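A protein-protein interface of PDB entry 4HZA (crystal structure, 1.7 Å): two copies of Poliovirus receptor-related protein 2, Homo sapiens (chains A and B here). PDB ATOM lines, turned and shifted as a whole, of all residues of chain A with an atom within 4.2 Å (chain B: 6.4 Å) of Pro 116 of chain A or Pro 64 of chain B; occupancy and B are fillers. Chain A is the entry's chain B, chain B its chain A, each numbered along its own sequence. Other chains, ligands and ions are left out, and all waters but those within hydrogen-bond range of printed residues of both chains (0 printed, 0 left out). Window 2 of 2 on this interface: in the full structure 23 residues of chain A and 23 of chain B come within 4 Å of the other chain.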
ATOM      1  N   MET A   1       7.762  33.579   0.398  1.00  0.00           N
ATOM      2  CA  MET A   1       6.506  33.533  -0.411  1.00  0.00           C
ATOM      3  C   MET A   1       5.297  34.047   0.397  1.00  0.00           C
ATOM      4  O   MET A   1       4.957  33.495   1.469  1.00  0.00           O
ATOM      5  CB  MET A   1       6.272  32.106  -0.891  1.00  0.00           C
ATOM      6  CG  MET A   1       5.597  32.021  -2.222  1.00  0.00           C
ATOM      7  SD  MET A   1       5.410  30.364  -2.941  1.00  0.00           S
ATOM      8  CE  MET A   1       7.028  30.024  -3.645  1.00  0.00           C
ATOM      9  N   LEU A  33       5.484  30.470  -7.254  1.00  0.00           N
ATOM     10  CA  LEU A  33       4.173  29.815  -7.135  1.00  0.00           C
ATOM     11  C   LEU A  33       3.682  29.170  -8.452  1.00  0.00           C
ATOM     12  O   LEU A  33       3.505  29.865  -9.424  1.00  0.00           O
ATOM     13  CB  LEU A  33       3.145  30.811  -6.572  1.00  0.00           C
ATOM     14  CG  LEU A  33       1.804  30.111  -6.206  1.00  0.00           C
ATOM     15  CD1 LEU A  33       1.976  29.070  -5.121  1.00  0.00           C
ATOM     16  CD2 LEU A  33       0.817  31.137  -5.719  1.00  0.00           C
ATOM     17  N   PHE A 115       1.068  24.978  -6.108  1.00  0.00           N
ATOM     18  CA  PHE A 115       2.179  24.319  -5.371  1.00  0.00           C
ATOM     19  C   PHE A 115       3.259  25.379  -5.143  1.00  0.00           C
ATOM     20  O   PHE A 115       3.662  26.051  -6.102  1.00  0.00           O
ATOM     21  CB  PHE A 115       2.752  23.126  -6.189  1.00  0.00           C
ATOM     22  CG  PHE A 115       3.799  22.362  -5.433  1.00  0.00           C
ATOM     23  CD1 PHE A 115       3.437  21.323  -4.615  1.00  0.00           C
ATOM     24  CD2 PHE A 115       5.133  22.730  -5.495  1.00  0.00           C
ATOM     25  CE1 PHE A 115       4.420  20.614  -3.920  1.00  0.00           C
ATOM     26  CE2 PHE A 115       6.105  22.027  -4.779  1.00  0.00           C
ATOM     27  CZ  PHE A 115       5.763  21.016  -4.012  1.00  0.00           C
ATOM     28  N   PRO A 116       3.816  25.487  -3.935  1.00  0.00           N
ATOM     29  CA  PRO A 116       3.715  24.675  -2.757  1.00  0.00           C
ATOM     30  C   PRO A 116       2.570  25.013  -1.845  1.00  0.00           C
ATOM     31  O   PRO A 116       2.386  24.320  -0.916  1.00  0.00           O
ATOM     32  CB  PRO A 116       5.078  24.914  -2.014  1.00  0.00           C
ATOM     33  CG  PRO A 116       5.410  26.273  -2.394  1.00  0.00           C
ATOM     34  CD  PRO A 116       4.705  26.630  -3.738  1.00  0.00           C
ATOM     35  N   LYS A 117       1.749  26.041  -2.170  1.00  0.00           N
ATOM     36  CA  LYS A 117       0.845  26.572  -1.150  1.00  0.00           C
ATOM     37  C   LYS A 117      -0.490  25.808  -0.994  1.00  0.00           C
ATOM     38  O   LYS A 117      -1.167  25.974   0.014  1.00  0.00           O
ATOM     39  CB  LYS A 117       0.574  28.077  -1.446  1.00  0.00           C
ATOM     40  CG  LYS A 117       1.841  28.993  -1.436  1.00  0.00           C
ATOM     41  CD  LYS A 117       1.903  29.817  -0.130  1.00  0.00           C
ATOM     42  CE  LYS A 117       3.335  30.092   0.359  1.00  0.00           C
ATOM     43  NZ  LYS A 117       3.398  30.631   1.756  1.00  0.00           N
ATOM     44  N   GLY A 118      -0.878  25.013  -1.988  1.00  0.00           N
ATOM     45  CA  GLY A 118      -2.100  24.187  -1.931  1.00  0.00           C
ATOM     46  C   GLY A 118      -3.276  24.848  -2.679  1.00  0.00           C
ATOM     47  O   GLY A 118      -3.076  25.669  -3.572  1.00  0.00           O
ATOM     48  N   ASN B  48      -4.596  30.774   6.742  1.00  0.00           N
ATOM     49  CA  ASN B  48      -3.164  30.600   6.474  1.00  0.00           C
ATOM     50  C   ASN B  48      -2.570  29.270   7.029  1.00  0.00           C
ATOM     51  O   ASN B  48      -1.365  28.965   6.858  1.00  0.00           O
ATOM     52  CB  ASN B  48      -2.393  31.847   6.931  1.00  0.00           C
ATOM     53  CG  ASN B  48      -2.026  31.819   8.383  1.00  0.00           C
ATOM     54  OD1 ASN B  48      -2.590  31.059   9.194  1.00  0.00           O
ATOM     55  ND2 ASN B  48      -1.059  32.676   8.746  1.00  0.00           N
ATOM     56  N   ASN B  51      -4.239  24.843   4.356  1.00  0.00           N
ATOM     57  CA  ASN B  51      -3.494  23.856   3.524  1.00  0.00           C
ATOM     58  C   ASN B  51      -2.384  23.227   4.310  1.00  0.00           C
ATOM     59  O   ASN B  51      -1.524  23.943   4.798  1.00  0.00           O
ATOM     60  CB  ASN B  51      -2.922  24.550   2.344  1.00  0.00           C
ATOM     61  CG  ASN B  51      -3.973  24.748   1.278  1.00  0.00           C
ATOM     62  OD1 ASN B  51      -4.361  23.740   0.613  1.00  0.00           O
ATOM     63  ND2 ASN B  51      -4.387  25.995   1.070  1.00  0.00           N
ATOM     64  N   VAL B  52      -2.497  21.931   4.522  1.00  0.00           N
ATOM     65  CA  VAL B  52      -1.472  21.240   5.370  1.00  0.00           C
ATOM     66  C   VAL B  52      -0.537  20.330   4.643  1.00  0.00           C
ATOM     67  O   VAL B  52       0.528  19.918   5.192  1.00  0.00           O
ATOM     68  CB  VAL B  52      -2.090  20.470   6.630  1.00  0.00           C
ATOM     69  CG1 VAL B  52      -2.794  21.441   7.513  1.00  0.00           C
ATOM     70  CG2 VAL B  52      -3.018  19.347   6.213  1.00  0.00           C
ATOM     71  N   ALA B  53      -0.904  19.924   3.437  1.00  0.00           N
ATOM     72  CA  ALA B  53      -0.050  18.971   2.669  1.00  0.00           C
ATOM     73  C   ALA B  53      -0.399  19.066   1.212  1.00  0.00           C
ATOM     74  O   ALA B  53      -1.589  19.296   0.892  1.00  0.00           O
ATOM     75  CB  ALA B  53      -0.157  17.479   3.198  1.00  0.00           C
ATOM     76  N   ALA B  54       0.581  19.052   0.304  1.00  0.00           N
ATOM     77  CA  ALA B  54       0.243  19.047  -1.123  1.00  0.00           C
ATOM     78  C   ALA B  54       1.217  18.129  -1.763  1.00  0.00           C
ATOM     79  O   ALA B  54       2.383  18.017  -1.283  1.00  0.00           O
ATOM     80  CB  ALA B  54       0.409  20.443  -1.771  1.00  0.00           C
ATOM     81  N   PRO B  61       6.388  16.566  -2.496  1.00  0.00           N
ATOM     82  CA  PRO B  61       5.579  17.076  -1.369  1.00  0.00           C
ATOM     83  C   PRO B  61       5.902  18.492  -0.894  1.00  0.00           C
ATOM     84  O   PRO B  61       7.027  18.995  -1.110  1.00  0.00           O
ATOM     85  CB  PRO B  61       5.968  16.118  -0.222  1.00  0.00           C
ATOM     86  CG  PRO B  61       7.430  15.910  -0.495  1.00  0.00           C
ATOM     87  CD  PRO B  61       7.489  15.717  -1.993  1.00  0.00           C
ATOM     88  N   SER B  62       4.901  19.149  -0.319  1.00  0.00           N
ATOM     89  CA  SER B  62       5.089  20.388   0.419  1.00  0.00           C
ATOM     90  C   SER B  62       4.118  20.355   1.614  1.00  0.00           C
ATOM     91  O   SER B  62       2.958  19.930   1.476  1.00  0.00           O
ATOM     92  CB  SER B  62       4.717  21.560  -0.470  1.00  0.00           C
ATOM     93  OG  SER B  62       3.340  21.707  -0.418  1.00  0.00           O
ATOM     94  N   PHE B  63       4.539  20.872   2.745  1.00  0.00           N
ATOM     95  CA  PHE B  63       3.727  20.845   3.959  1.00  0.00           C
ATOM     96  C   PHE B  63       3.749  22.285   4.411  1.00  0.00           C
ATOM     97  O   PHE B  63       4.705  22.672   5.101  1.00  0.00           O
ATOM     98  CB  PHE B  63       4.374  19.898   4.992  1.00  0.00           C
ATOM     99  CG  PHE B  63       4.464  18.461   4.496  1.00  0.00           C
ATOM    100  CD1 PHE B  63       3.318  17.694   4.309  1.00  0.00           C
ATOM    101  CD2 PHE B  63       5.689  17.902   4.220  1.00  0.00           C
ATOM    102  CE1 PHE B  63       3.432  16.385   3.838  1.00  0.00           C
ATOM    103  CE2 PHE B  63       5.818  16.572   3.782  1.00  0.00           C
ATOM    104  CZ  PHE B  63       4.696  15.838   3.551  1.00  0.00           C
ATOM    105  N   PRO B  64       2.785  23.090   3.884  1.00  0.00           N
ATOM    106  CA  PRO B  64       2.937  24.542   3.979  1.00  0.00           C
ATOM    107  C   PRO B  64       2.580  25.103   5.366  1.00  0.00           C
ATOM    108  O   PRO B  64       3.086  26.204   5.717  1.00  0.00           O
ATOM    109  CB  PRO B  64       2.047  25.058   2.810  1.00  0.00           C
ATOM    110  CG  PRO B  64       1.030  24.041   2.621  1.00  0.00           C
ATOM    111  CD  PRO B  64       1.765  22.716   2.901  1.00  0.00           C
ATOM    112  N   SER B  65       1.852  24.343   6.196  1.00  0.00           N
ATOM    113  CA  SER B  65       1.309  24.854   7.485  1.00  0.00           C
ATOM    114  C   SER B  65       2.194  24.406   8.668  1.00  0.00           C
ATOM    115  O   SER B  65       2.803  23.350   8.607  1.00  0.00           O
ATOM    116  CB  SER B  65      -0.120  24.300   7.664  1.00  0.00           C
ATOM    117  OG  SER B  65      -0.655  24.432   8.989  1.00  0.00           O
ATOM    118  N   PRO B  66       2.246  25.187   9.755  1.00  0.00           N
ATOM    119  CA  PRO B  66       2.836  24.592  10.996  1.00  0.00           C
ATOM    120  C   PRO B  66       1.958  23.532  11.720  1.00  0.00           C
ATOM    121  O   PRO B  66       2.413  22.830  12.623  1.00  0.00           O
ATOM    122  CB  PRO B  66       3.090  25.822  11.887  1.00  0.00           C
ATOM    123  CG  PRO B  66       3.149  27.047  10.864  1.00  0.00           C
ATOM    124  CD  PRO B  66       2.070  26.658   9.857  1.00  0.00           C
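ND2 of Asn 51 of chain B sits close to O of Lys 117 of chain A, 3.4 Å away. OG of Ser 62 of chain B is in hydrogen-bond range of O of Pro 116 of chain A.
The backbone carbonyl oxygen (O) of Ser 62 of chain B sits at hydrogen-bond distance from the backbone NH (N) of Ala 54 of chain B, 2.8 Å away. O of Met 1 of chain A sits at hydrogen-bond distance from NZ of Lys 117 of chain A, at 3.3 Å.
CZ of Phe 115 of chain A touches O of Pro 61 of chain B (3.8 Å). CB of Ser 62 of chain B touches CE1 of Phe 115 of chain A (3.6 Å). Pro 116 of chain A touches Pro 64 of chain B (O to CG, 3.8 Å). Lys 117 of chain A touches Pro 64 of chain B. OD1 of Asn 51 of chain B touches CA of Gly 118 of chain A, at 3.4 Å.
Printed residues of chain B within 4 Å of Pro 116 of chain A: Ser 62 and Pro 64. Of the printed residues of chain A, Pro 64 of chain B touches Pro 116 and Lys 117. Printed residues of chain B within 4 Å of Gly 118 of chain A: Asn 51 (3.4 Å). Of the printed residues of chain A, Asn 51 of chain B touches Lys 117 (3.2 Å) and Gly 118 (3.4 Å). Of the printed residues of chain A, Ser 62 of chain B touches Phe 115 (3.6 Å) and Pro 116 (2.8 Å). Of the printed residues of chain A, Pro 61 of chain B touches Phe 115. Printed residues of chain B within 4 Å of Phe 115 of chain A: Pro 61 (3.8 Å) and Ser 62 (3.6 Å). Pro 66 of chain B touches none of the printed residues of chain A. The nearest printed residue of chain A that does not touch Pro 64 of chain B is Gly 118 of chain A (5.1 Å). The nearest printed residue of chain B that does not touch Lys 117 of chain A is Ser 62 of chain B (4.9 Å).
Of the 11 printed residues of chain B, 4 touch a printed residue of chain A. Hydrophobic or aromatic side chains of chain B within 4 Å of the printed part of chain A: Pro 64. Printed residues of chain A that touch a printed residue of chain B: Phe 115, Pro 116, Lys 117 and Gly 118. Hydrophobic or aromatic side chains of chain A that line the printed part of chain B: Phe 115 and Pro 116. Among the printed residues, 7 pairs touch across the chains. Among the printed residues, no Asp or Glu carboxylate lies within 4 Å of a Lys or Arg side-chain nitrogen of the other chain.
No position is printed for both chains. Of the 7 pairs that touch across the chains among the printed residues, none has its exchanged pair printed and touching as well.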
